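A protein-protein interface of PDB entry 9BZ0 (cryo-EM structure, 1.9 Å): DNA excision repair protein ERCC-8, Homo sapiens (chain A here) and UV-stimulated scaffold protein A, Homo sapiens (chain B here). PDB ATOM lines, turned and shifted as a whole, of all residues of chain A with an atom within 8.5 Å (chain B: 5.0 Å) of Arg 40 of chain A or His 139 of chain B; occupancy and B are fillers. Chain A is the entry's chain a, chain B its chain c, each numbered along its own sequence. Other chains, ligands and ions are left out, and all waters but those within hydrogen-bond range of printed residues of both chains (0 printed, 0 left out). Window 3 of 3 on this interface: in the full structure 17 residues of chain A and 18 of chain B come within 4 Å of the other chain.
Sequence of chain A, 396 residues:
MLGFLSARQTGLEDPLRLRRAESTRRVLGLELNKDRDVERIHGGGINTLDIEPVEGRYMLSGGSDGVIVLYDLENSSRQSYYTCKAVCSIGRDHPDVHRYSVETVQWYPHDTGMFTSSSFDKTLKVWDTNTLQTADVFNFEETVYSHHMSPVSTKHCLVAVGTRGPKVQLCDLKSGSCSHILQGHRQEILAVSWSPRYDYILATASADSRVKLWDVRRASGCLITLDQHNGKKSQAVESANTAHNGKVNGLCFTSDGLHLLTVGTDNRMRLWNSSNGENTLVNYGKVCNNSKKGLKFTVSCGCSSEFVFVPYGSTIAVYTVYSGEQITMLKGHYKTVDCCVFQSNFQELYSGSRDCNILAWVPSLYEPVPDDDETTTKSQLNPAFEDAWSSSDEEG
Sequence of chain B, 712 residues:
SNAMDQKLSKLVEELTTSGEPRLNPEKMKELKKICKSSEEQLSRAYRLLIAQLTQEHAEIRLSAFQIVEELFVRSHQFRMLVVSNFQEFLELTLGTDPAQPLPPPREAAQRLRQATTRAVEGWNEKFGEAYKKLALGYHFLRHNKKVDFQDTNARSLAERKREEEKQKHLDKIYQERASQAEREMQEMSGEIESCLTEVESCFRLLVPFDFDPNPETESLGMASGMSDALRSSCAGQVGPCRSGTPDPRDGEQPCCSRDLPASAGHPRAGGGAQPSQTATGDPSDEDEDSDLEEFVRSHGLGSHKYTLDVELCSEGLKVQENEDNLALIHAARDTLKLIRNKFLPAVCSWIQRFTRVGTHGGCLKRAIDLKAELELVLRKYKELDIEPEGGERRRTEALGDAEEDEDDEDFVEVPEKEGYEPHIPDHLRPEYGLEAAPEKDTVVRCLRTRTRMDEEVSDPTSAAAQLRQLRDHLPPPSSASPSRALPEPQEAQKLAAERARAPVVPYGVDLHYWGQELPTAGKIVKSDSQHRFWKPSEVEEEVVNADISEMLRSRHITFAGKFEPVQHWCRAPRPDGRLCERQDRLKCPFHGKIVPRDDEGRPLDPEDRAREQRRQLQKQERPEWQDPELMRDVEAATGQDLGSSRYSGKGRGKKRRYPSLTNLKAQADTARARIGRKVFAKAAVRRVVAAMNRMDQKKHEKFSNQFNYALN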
ATOM      1  N   ASN A  33      25.787  -5.646  -6.358  1.00  0.00           N
ATOM      2  CA  ASN A  33      26.674  -6.774  -6.662  1.00  0.00           C
ATOM      3  C   ASN A  33      27.623  -6.504  -7.817  1.00  0.00           C
ATOM      4  O   ASN A  33      27.954  -7.419  -8.567  1.00  0.00           O
ATOM      5  CB  ASN A  33      25.894  -8.058  -6.941  1.00  0.00           C
ATOM      6  CG  ASN A  33      25.209  -8.609  -5.723  1.00  0.00           C
ATOM      7  OD1 ASN A  33      23.997  -8.776  -5.705  1.00  0.00           O
ATOM      8  ND2 ASN A  33      25.983  -8.933  -4.708  1.00  0.00           N
ATOM      9  N   ASP A  37      29.662 -11.105  -5.288  1.00  0.00           N
ATOM     10  CA  ASP A  37      28.614 -11.880  -4.643  1.00  0.00           C
ATOM     11  C   ASP A  37      28.959 -12.149  -3.187  1.00  0.00           C
ATOM     12  O   ASP A  37      30.098 -11.994  -2.752  1.00  0.00           O
ATOM     13  CB  ASP A  37      28.407 -13.203  -5.379  1.00  0.00           C
ATOM     14  CG  ASP A  37      27.663 -13.036  -6.673  1.00  0.00           C
ATOM     15  OD1 ASP A  37      26.489 -12.614  -6.635  1.00  0.00           O
ATOM     16  OD2 ASP A  37      28.248 -13.329  -7.738  1.00  0.00           O
ATOM     17  N   VAL A  38      27.951 -12.566  -2.432  1.00  0.00           N
ATOM     18  CA  VAL A  38      28.127 -13.181  -1.124  1.00  0.00           C
ATOM     19  C   VAL A  38      27.590 -14.603  -1.178  1.00  0.00           C
ATOM     20  O   VAL A  38      26.489 -14.834  -1.686  1.00  0.00           O
ATOM     21  CB  VAL A  38      27.437 -12.360  -0.023  1.00  0.00           C
ATOM     22  CG1 VAL A  38      27.685 -12.974   1.329  1.00  0.00           C
ATOM     23  CG2 VAL A  38      27.944 -10.940  -0.046  1.00  0.00           C
ATOM     24  N   GLU A  39      28.363 -15.548  -0.661  1.00  0.00           N
ATOM     25  CA  GLU A  39      28.019 -16.963  -0.735  1.00  0.00           C
ATOM     26  C   GLU A  39      26.732 -17.266   0.022  1.00  0.00           C
ATOM     27  O   GLU A  39      26.588 -16.898   1.189  1.00  0.00           O
ATOM     28  CB  GLU A  39      29.171 -17.786  -0.169  1.00  0.00           C
ATOM     29  CG  GLU A  39      28.958 -19.274  -0.193  1.00  0.00           C
ATOM     30  CD  GLU A  39      30.222 -20.040   0.108  1.00  0.00           C
ATOM     31  OE1 GLU A  39      31.007 -19.583   0.959  1.00  0.00           O
ATOM     32  OE2 GLU A  39      30.436 -21.103  -0.508  1.00  0.00           O
ATOM     33  N   ARG A  40      25.790 -17.940  -0.640  1.00  0.00           N
ATOM     34  CA  ARG A  40      24.528 -18.339  -0.010  1.00  0.00           C
ATOM     35  C   ARG A  40      24.735 -19.547   0.890  1.00  0.00           C
ATOM     36  O   ARG A  40      24.719 -20.684   0.427  1.00  0.00           O
ATOM     37  CB  ARG A  40      23.479 -18.678  -1.057  1.00  0.00           C
ATOM     38  CG  ARG A  40      22.928 -17.532  -1.850  1.00  0.00           C
ATOM     39  CD  ARG A  40      21.791 -18.038  -2.717  1.00  0.00           C
ATOM     40  NE  ARG A  40      21.256 -17.011  -3.596  1.00  0.00           N
ATOM     41  CZ  ARG A  40      21.775 -16.693  -4.773  1.00  0.00           C
ATOM     42  NH1 ARG A  40      21.273 -15.664  -5.448  1.00  0.00           N
ATOM     43  NH2 ARG A  40      22.747 -17.409  -5.313  1.00  0.00           N
ATOM     44  N   ILE A  41      24.924 -19.319   2.183  1.00  0.00           N
ATOM     45  CA  ILE A  41      24.957 -20.399   3.157  1.00  0.00           C
ATOM     46  C   ILE A  41      23.621 -20.572   3.867  1.00  0.00           C
ATOM     47  O   ILE A  41      23.184 -21.697   4.103  1.00  0.00           O
ATOM     48  CB  ILE A  41      26.103 -20.180   4.163  1.00  0.00           C
ATOM     49  CG1 ILE A  41      27.437 -20.170   3.431  1.00  0.00           C
ATOM     50  CG2 ILE A  41      26.103 -21.253   5.209  1.00  0.00           C
ATOM     51  CD1 ILE A  41      27.698 -21.423   2.659  1.00  0.00           C
ATOM     52  N   HIS A  42      22.963 -19.475   4.209  1.00  0.00           N
ATOM     53  CA  HIS A  42      21.707 -19.534   4.938  1.00  0.00           C
ATOM     54  C   HIS A  42      20.597 -20.152   4.099  1.00  0.00           C
ATOM     55  O   HIS A  42      20.541 -19.985   2.880  1.00  0.00           O
ATOM     56  CB  HIS A  42      21.289 -18.140   5.386  1.00  0.00           C
ATOM     57  CG  HIS A  42      22.052 -17.620   6.561  1.00  0.00           C
ATOM     58  ND1 HIS A  42      21.785 -18.009   7.854  1.00  0.00           N
ATOM     59  CD2 HIS A  42      23.060 -16.723   6.641  1.00  0.00           C
ATOM     60  CE1 HIS A  42      22.601 -17.380   8.678  1.00  0.00           C
ATOM     61  NE2 HIS A  42      23.381 -16.590   7.967  1.00  0.00           N
ATOM     62  N   GLY A  43      19.705 -20.869   4.772  1.00  0.00           N
ATOM     63  CA  GLY A  43      18.456 -21.284   4.174  1.00  0.00           C
ATOM     64  C   GLY A  43      17.285 -20.407   4.557  1.00  0.00           C
ATOM     65  O   GLY A  43      16.243 -20.426   3.901  1.00  0.00           O
ATOM     66  N   ILE A  46      17.997 -13.438   6.597  1.00  0.00           N
ATOM     67  CA  ILE A  46      19.149 -12.869   7.285  1.00  0.00           C
ATOM     68  C   ILE A  46      18.655 -11.799   8.247  1.00  0.00           C
ATOM     69  O   ILE A  46      18.334 -10.686   7.842  1.00  0.00           O
ATOM     70  CB  ILE A  46      20.159 -12.291   6.301  1.00  0.00           C
ATOM     71  CG1 ILE A  46      20.375 -13.252   5.145  1.00  0.00           C
ATOM     72  CG2 ILE A  46      21.451 -11.991   7.009  1.00  0.00           C
ATOM     73  CD1 ILE A  46      20.932 -14.513   5.538  1.00  0.00           C
ATOM     74  N   VAL A  69      26.840 -17.477  10.475  1.00  0.00           N
ATOM     75  CA  VAL A  69      27.847 -17.637   9.434  1.00  0.00           C
ATOM     76  C   VAL A  69      28.866 -16.517   9.559  1.00  0.00           C
ATOM     77  O   VAL A  69      28.505 -15.365   9.811  1.00  0.00           O
ATOM     78  CB  VAL A  69      27.222 -17.658   8.029  1.00  0.00           C
ATOM     79  CG1 VAL A  69      28.270 -17.991   7.002  1.00  0.00           C
ATOM     80  CG2 VAL A  69      26.099 -18.652   7.972  1.00  0.00           C
ATOM     81  N   TYR A  71      31.847 -14.616   7.423  1.00  0.00           N
ATOM     82  CA  TYR A  71      32.279 -14.362   6.058  1.00  0.00           C
ATOM     83  C   TYR A  71      33.570 -13.558   6.025  1.00  0.00           C
ATOM     84  O   TYR A  71      33.809 -12.709   6.882  1.00  0.00           O
ATOM     85  CB  TYR A  71      31.240 -13.564   5.286  1.00  0.00           C
ATOM     86  CG  TYR A  71      29.971 -14.270   4.949  1.00  0.00           C
ATOM     87  CD1 TYR A  71      29.877 -15.075   3.844  1.00  0.00           C
ATOM     88  CD2 TYR A  71      28.839 -14.061   5.700  1.00  0.00           C
ATOM     89  CE1 TYR A  71      28.720 -15.705   3.540  1.00  0.00           C
ATOM     90  CE2 TYR A  71      27.676 -14.673   5.390  1.00  0.00           C
ATOM     91  CZ  TYR A  71      27.620 -15.494   4.311  1.00  0.00           C
ATOM     92  OH  TYR A  71      26.440 -16.102   3.983  1.00  0.00           O
ATOM     93  N   THR A  83      33.707 -13.865  -4.983  1.00  0.00           N
ATOM     94  CA  THR A  83      32.706 -14.253  -4.001  1.00  0.00           C
ATOM     95  C   THR A  83      33.235 -14.046  -2.593  1.00  0.00           C
ATOM     96  O   THR A  83      34.331 -14.506  -2.270  1.00  0.00           O
ATOM     97  CB  THR A  83      32.308 -15.711  -4.192  1.00  0.00           C
ATOM     98  OG1 THR A  83      31.750 -15.882  -5.496  1.00  0.00           O
ATOM     99  CG2 THR A  83      31.290 -16.114  -3.169  1.00  0.00           C
ATOM    100  N   CYS A  84      32.459 -13.367  -1.757  1.00  0.00           N
ATOM    101  CA  CYS A  84      32.703 -13.338  -0.317  1.00  0.00           C
ATOM    102  C   CYS A  84      32.358 -14.691   0.284  1.00  0.00           C
ATOM    103  O   CYS A  84      31.191 -15.022   0.483  1.00  0.00           O
ATOM    104  CB  CYS A  84      31.909 -12.218   0.337  1.00  0.00           C
ATOM    105  SG  CYS A  84      32.156 -10.600  -0.393  1.00  0.00           S
ATOM    106  N   LYS A  85      33.386 -15.472   0.581  1.00  0.00           N
ATOM    107  CA  LYS A  85      33.228 -16.846   1.018  1.00  0.00           C
ATOM    108  C   LYS A  85      32.982 -16.939   2.513  1.00  0.00           C
ATOM    109  O   LYS A  85      33.413 -16.087   3.291  1.00  0.00           O
ATOM    110  CB  LYS A  85      34.453 -17.663   0.632  1.00  0.00           C
ATOM    111  CG  LYS A  85      34.507 -17.987  -0.843  1.00  0.00           C
ATOM    112  CD  LYS A  85      35.707 -18.845  -1.177  1.00  0.00           C
ATOM    113  CE  LYS A  85      35.724 -19.209  -2.650  1.00  0.00           C
ATOM    114  NZ  LYS A  85      36.908 -20.039  -3.002  1.00  0.00           N
ATOM    115  N   ALA A  86      32.270 -17.987   2.912  1.00  0.00           N
ATOM    116  CA  ALA A  86      32.083 -18.300   4.321  1.00  0.00           C
ATOM    117  C   ALA A  86      33.304 -18.993   4.899  1.00  0.00           C
ATOM    118  O   ALA A  86      33.681 -20.079   4.457  1.00  0.00           O
ATOM    119  CB  ALA A  86      30.849 -19.172   4.499  1.00  0.00           C
ATOM    120  N   TYR A 334      14.016  -9.159  -2.790  1.00  0.00           N
ATOM    121  CA  TYR A 334      12.670  -9.596  -3.148  1.00  0.00           C
ATOM    122  C   TYR A 334      11.713  -9.692  -1.969  1.00  0.00           C
ATOM    123  O   TYR A 334      10.515  -9.882  -2.185  1.00  0.00           O
ATOM    124  CB  TYR A 334      12.711 -10.934  -3.876  1.00  0.00           C
ATOM    125  CG  TYR A 334      13.155 -10.745  -5.281  1.00  0.00           C
ATOM    126  CD1 TYR A 334      12.249 -10.445  -6.268  1.00  0.00           C
ATOM    127  CD2 TYR A 334      14.481 -10.831  -5.619  1.00  0.00           C
ATOM    128  CE1 TYR A 334      12.646 -10.272  -7.554  1.00  0.00           C
ATOM    129  CE2 TYR A 334      14.889 -10.638  -6.900  1.00  0.00           C
ATOM    130  CZ  TYR A 334      13.967 -10.357  -7.864  1.00  0.00           C
ATOM    131  OH  TYR A 334      14.372 -10.140  -9.155  1.00  0.00           O
ATOM    132  N   ASP A 355      14.451 -12.733   1.943  1.00  0.00           N
ATOM    133  CA  ASP A 355      14.688 -13.477   0.715  1.00  0.00           C
ATOM    134  C   ASP A 355      15.937 -14.342   0.770  1.00  0.00           C
ATOM    135  O   ASP A 355      16.295 -14.942  -0.245  1.00  0.00           O
ATOM    136  CB  ASP A 355      14.727 -12.519  -0.481  1.00  0.00           C
ATOM    137  CG  ASP A 355      15.992 -11.684  -0.551  1.00  0.00           C
ATOM    138  OD1 ASP A 355      16.900 -11.828   0.289  1.00  0.00           O
ATOM    139  OD2 ASP A 355      16.081 -10.860  -1.480  1.00  0.00           O
ATOM    140  N   CYS A 356      16.602 -14.404   1.915  1.00  0.00           N
ATOM    141  CA  CYS A 356      17.794 -15.187   2.203  1.00  0.00           C
ATOM    142  C   CYS A 356      19.050 -14.712   1.488  1.00  0.00           C
ATOM    143  O   CYS A 356      20.103 -15.313   1.692  1.00  0.00           O
ATOM    144  CB  CYS A 356      17.595 -16.675   1.894  1.00  0.00           C
ATOM    145  SG  CYS A 356      16.037 -17.351   2.486  1.00  0.00           S
ATOM    146  N   ASN A 357      18.989 -13.680   0.659  1.00  0.00           N
ATOM    147  CA  ASN A 357      20.215 -13.140   0.102  1.00  0.00           C
ATOM    148  C   ASN A 357      20.880 -12.190   1.084  1.00  0.00           C
ATOM    149  O   ASN A 357      20.214 -11.470   1.828  1.00  0.00           O
ATOM    150  CB  ASN A 357      19.950 -12.405  -1.204  1.00  0.00           C
ATOM    151  CG  ASN A 357      19.321 -13.274  -2.236  1.00  0.00           C
ATOM    152  OD1 ASN A 357      19.906 -14.263  -2.665  1.00  0.00           O
ATOM    153  ND2 ASN A 357      18.131 -12.906  -2.669  1.00  0.00           N
ATOM    154  N   ILE A 358      22.206 -12.193   1.083  1.00  0.00           N
ATOM    155  CA  ILE A 358      22.999 -11.038   1.474  1.00  0.00           C
ATOM    156  C   ILE A 358      23.507 -10.395   0.197  1.00  0.00           C
ATOM    157  O   ILE A 358      24.172 -11.047  -0.612  1.00  0.00           O
ATOM    158  CB  ILE A 358      24.149 -11.430   2.409  1.00  0.00           C
ATOM    159  CG1 ILE A 358      23.600 -12.112   3.649  1.00  0.00           C
ATOM    160  CG2 ILE A 358      24.911 -10.206   2.838  1.00  0.00           C
ATOM    161  CD1 ILE A 358      24.642 -12.708   4.508  1.00  0.00           C
ATOM    162  N   LEU A 359      23.190  -9.125   0.007  1.00  0.00           N
ATOM    163  CA  LEU A 359      23.580  -8.369  -1.171  1.00  0.00           C
ATOM    164  C   LEU A 359      24.611  -7.307  -0.827  1.00  0.00           C
ATOM    165  O   LEU A 359      24.499  -6.627   0.193  1.00  0.00           O
ATOM    166  CB  LEU A 359      22.368  -7.722  -1.829  1.00  0.00           C
ATOM    167  CG  LEU A 359      21.275  -8.675  -2.297  1.00  0.00           C
ATOM    168  CD1 LEU A 359      20.140  -7.913  -2.921  1.00  0.00           C
ATOM    169  CD2 LEU A 359      21.839  -9.662  -3.266  1.00  0.00           C
ATOM    170  N   ALA B 135      18.814 -12.648 -12.364  1.00  0.00           N
ATOM    171  CA  ALA B 135      19.300 -13.916 -11.833  1.00  0.00           C
ATOM    172  C   ALA B 135      18.871 -14.133 -10.390  1.00  0.00           C
ATOM    173  O   ALA B 135      18.486 -15.248 -10.011  1.00  0.00           O
ATOM    174  CB  ALA B 135      20.817 -13.979 -11.948  1.00  0.00           C
ATOM    175  N   LEU B 136      18.893 -13.075  -9.577  1.00  0.00           N
ATOM    176  CA  LEU B 136      18.347 -13.185  -8.227  1.00  0.00           C
ATOM    177  C   LEU B 136      16.872 -13.548  -8.242  1.00  0.00           C
ATOM    178  O   LEU B 136      16.422 -14.368  -7.436  1.00  0.00           O
ATOM    179  CB  LEU B 136      18.562 -11.884  -7.461  1.00  0.00           C
ATOM    180  CG  LEU B 136      19.993 -11.468  -7.143  1.00  0.00           C
ATOM    181  CD1 LEU B 136      19.992 -10.131  -6.446  1.00  0.00           C
ATOM    182  CD2 LEU B 136      20.654 -12.505  -6.275  1.00  0.00           C
ATOM    183  N   GLY B 137      16.100 -12.939  -9.135  1.00  0.00           N
ATOM    184  CA  GLY B 137      14.688 -13.263  -9.229  1.00  0.00           C
ATOM    185  C   GLY B 137      14.432 -14.703  -9.615  1.00  0.00           C
ATOM    186  O   GLY B 137      13.564 -15.370  -9.046  1.00  0.00           O
ATOM    187  N   TYR B 138      15.172 -15.196 -10.602  1.00  0.00           N
ATOM    188  CA  TYR B 138      15.059 -16.599 -10.972  1.00  0.00           C
ATOM    189  C   TYR B 138      15.391 -17.519  -9.810  1.00  0.00           C
ATOM    190  O   TYR B 138      14.691 -18.510  -9.582  1.00  0.00           O
ATOM    191  CB  TYR B 138      15.972 -16.898 -12.157  1.00  0.00           C
ATOM    192  CG  TYR B 138      15.988 -18.351 -12.561  1.00  0.00           C
ATOM    193  CD1 TYR B 138      14.995 -18.876 -13.371  1.00  0.00           C
ATOM    194  CD2 TYR B 138      16.995 -19.199 -12.131  1.00  0.00           C
ATOM    195  CE1 TYR B 138      15.003 -20.199 -13.737  1.00  0.00           C
ATOM    196  CE2 TYR B 138      17.010 -20.525 -12.494  1.00  0.00           C
ATOM    197  CZ  TYR B 138      16.012 -21.019 -13.296  1.00  0.00           C
ATOM    198  OH  TYR B 138      16.028 -22.344 -13.666  1.00  0.00           O
ATOM    199  N   HIS B 139      16.456 -17.230  -9.075  1.00  0.00           N
ATOM    200  CA  HIS B 139      16.779 -18.067  -7.926  1.00  0.00           C
ATOM    201  C   HIS B 139      15.688 -18.020  -6.867  1.00  0.00           C
ATOM    202  O   HIS B 139      15.337 -19.046  -6.277  1.00  0.00           O
ATOM    203  CB  HIS B 139      18.109 -17.655  -7.317  1.00  0.00           C
ATOM    204  CG  HIS B 139      18.575 -18.569  -6.233  1.00  0.00           C
ATOM    205  ND1 HIS B 139      17.986 -18.610  -4.988  1.00  0.00           N
ATOM    206  CD2 HIS B 139      19.581 -19.473  -6.201  1.00  0.00           C
ATOM    207  CE1 HIS B 139      18.604 -19.504  -4.239  1.00  0.00           C
ATOM    208  NE2 HIS B 139      19.578 -20.041  -4.950  1.00  0.00           N
ATOM    209  N   PHE B 140      15.158 -16.832  -6.599  1.00  0.00           N
ATOM    210  CA  PHE B 140      14.043 -16.674  -5.675  1.00  0.00           C
ATOM    211  C   PHE B 140      12.841 -17.513  -6.067  1.00  0.00           C
ATOM    212  O   PHE B 140      12.278 -18.231  -5.235  1.00  0.00           O
ATOM    213  CB  PHE B 140      13.664 -15.201  -5.613  1.00  0.00           C
ATOM    214  CG  PHE B 140      12.442 -14.916  -4.812  1.00  0.00           C
ATOM    215  CD1 PHE B 140      12.466 -14.974  -3.441  1.00  0.00           C
ATOM    216  CD2 PHE B 140      11.279 -14.528  -5.436  1.00  0.00           C
ATOM    217  CE1 PHE B 140      11.341 -14.687  -2.713  1.00  0.00           C
ATOM    218  CE2 PHE B 140      10.160 -14.242  -4.713  1.00  0.00           C
ATOM    219  CZ  PHE B 140      10.190 -14.319  -3.353  1.00  0.00           C
ATOM    220  N   LEU B 141      12.475 -17.492  -7.345  1.00  0.00           N
ATOM    221  CA  LEU B 141      11.394 -18.352  -7.815  1.00  0.00           C
ATOM    222  C   LEU B 141      11.729 -19.820  -7.622  1.00  0.00           C
ATOM    223  O   LEU B 141      10.967 -20.565  -7.001  1.00  0.00           O
ATOM    224  CB  LEU B 141      11.094 -18.072  -9.281  1.00  0.00           C
ATOM    225  CG  LEU B 141      10.500 -16.709  -9.598  1.00  0.00           C
ATOM    226  CD1 LEU B 141      10.401 -16.530 -11.096  1.00  0.00           C
ATOM    227  CD2 LEU B 141       9.148 -16.548  -8.937  1.00  0.00           C
ATOM    228  N   ARG B 142      12.872 -20.252  -8.139  1.00  0.00           N
ATOM    229  CA  ARG B 142      13.180 -21.672  -8.194  1.00  0.00           C
ATOM    230  C   ARG B 142      13.333 -22.278  -6.807  1.00  0.00           C
ATOM    231  O   ARG B 142      12.911 -23.416  -6.576  1.00  0.00           O
ATOM    232  CB  ARG B 142      14.443 -21.896  -9.023  1.00  0.00           C
ATOM    233  CG  ARG B 142      14.830 -23.351  -9.190  1.00  0.00           C
ATOM    234  CD  ARG B 142      15.914 -23.514 -10.242  1.00  0.00           C
ATOM    235  NE  ARG B 142      16.364 -24.897 -10.350  1.00  0.00           N
ATOM    236  CZ  ARG B 142      17.091 -25.372 -11.352  1.00  0.00           C
ATOM    237  NH1 ARG B 142      17.461 -26.649 -11.336  1.00  0.00           N
ATOM    238  NH2 ARG B 142      17.449 -24.607 -12.370  1.00  0.00           N
ATOM    239  N   HIS B 143      13.920 -21.547  -5.869  1.00  0.00           N
ATOM    240  CA  HIS B 143      14.277 -22.121  -4.582  1.00  0.00           C
ATOM    241  C   HIS B 143      13.401 -21.678  -3.424  1.00  0.00           C
ATOM    242  O   HIS B 143      13.177 -22.474  -2.513  1.00  0.00           O
ATOM    243  CB  HIS B 143      15.740 -21.803  -4.255  1.00  0.00           C
ATOM    244  CG  HIS B 143      16.710 -22.392  -5.231  1.00  0.00           C
ATOM    245  ND1 HIS B 143      17.026 -23.734  -5.246  1.00  0.00           N
ATOM    246  CD2 HIS B 143      17.407 -21.831  -6.246  1.00  0.00           C
ATOM    247  CE1 HIS B 143      17.893 -23.969  -6.215  1.00  0.00           C
ATOM    248  NE2 HIS B 143      18.141 -22.830  -6.838  1.00  0.00           N
ATOM    249  N   ASN B 144      12.907 -20.446  -3.414  1.00  0.00           N
ATOM    250  CA  ASN B 144      12.234 -19.937  -2.228  1.00  0.00           C
ATOM    251  C   ASN B 144      10.721 -19.898  -2.357  1.00  0.00           C
ATOM    252  O   ASN B 144      10.024 -20.116  -1.363  1.00  0.00           O
ATOM    253  CB  ASN B 144      12.743 -18.531  -1.894  1.00  0.00           C
ATOM    254  CG  ASN B 144      14.231 -18.507  -1.598  1.00  0.00           C
ATOM    255  OD1 ASN B 144      14.824 -19.530  -1.255  1.00  0.00           O
ATOM    256  ND2 ASN B 144      14.841 -17.335  -1.731  1.00  0.00           N
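Among the printed residues, pairs that only touch across the chains: Arg 40 of chain A with Leu 136 of chain B (3.3 Å), Arg 40 of chain A with His 139 of chain B (3.7 Å), Leu 359 of chain A with Leu 136 of chain B (3.7 Å) and Tyr 334 of chain A with Leu 136 of chain B (3.8 Å).
ND2 of Asn 144 of chain B is in hydrogen-bond range of O of Asp 355 of chain A, 3.2 Å away. The side-chain hydroxyl (OH) of Tyr 334 of chain A sits close to the backbone NH (N) of Gly 137 of chain B (3.3 Å).
NE of Arg 40 of chain A is in hydrogen-bond range of OD1 of Asn 357 of chain A (3.2 Å). The backbone NH (N) of Tyr 334 of chain A sits at hydrogen-bond distance from the side-chain carboxylate (OD2) of Asp 355 of chain A. The side-chain carboxylate (OD1) of Asp 355 of chain A lies within hydrogen-bond range of the backbone NH (N) of Asn 357 of chain A (2.8 Å).
Of the 10 printed residues of chain B, 4 touch a printed residue of chain A. Of the 21 printed residues of chain A, 4 touch a printed residue of chain B. Hydrophobic or aromatic side chains of chain A that line the printed part of chain B: Tyr 334 and Leu 359.
Of the printed residues of chain B, Arg 40 of chain A touches Leu 136 (3.3 Å) and His 139 (3.7 Å). Of chain A, only Arg 40 (3.7 Å) comes within 4 Å of His 139 of chain B. Printed residues of chain A within 4 Å of Gly 137 of chain B: Tyr 334 (3.1 Å). Printed residues of chain B within 4 Å of Asp 355 of chain A: Asn 144 (3.2 Å). Of the printed residues of chain A, Leu 136 of chain B touches Arg 40, Tyr 334 and Leu 359. Of the printed residues of chain B, Tyr 334 of chain A touches Leu 136 and Gly 137. Of the printed residues of chain B, Leu 359 of chain A touches Leu 136. The nearest printed residue of chain B that does not touch Arg 40 of chain A is Ala 135 of chain B (5.4 Å).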
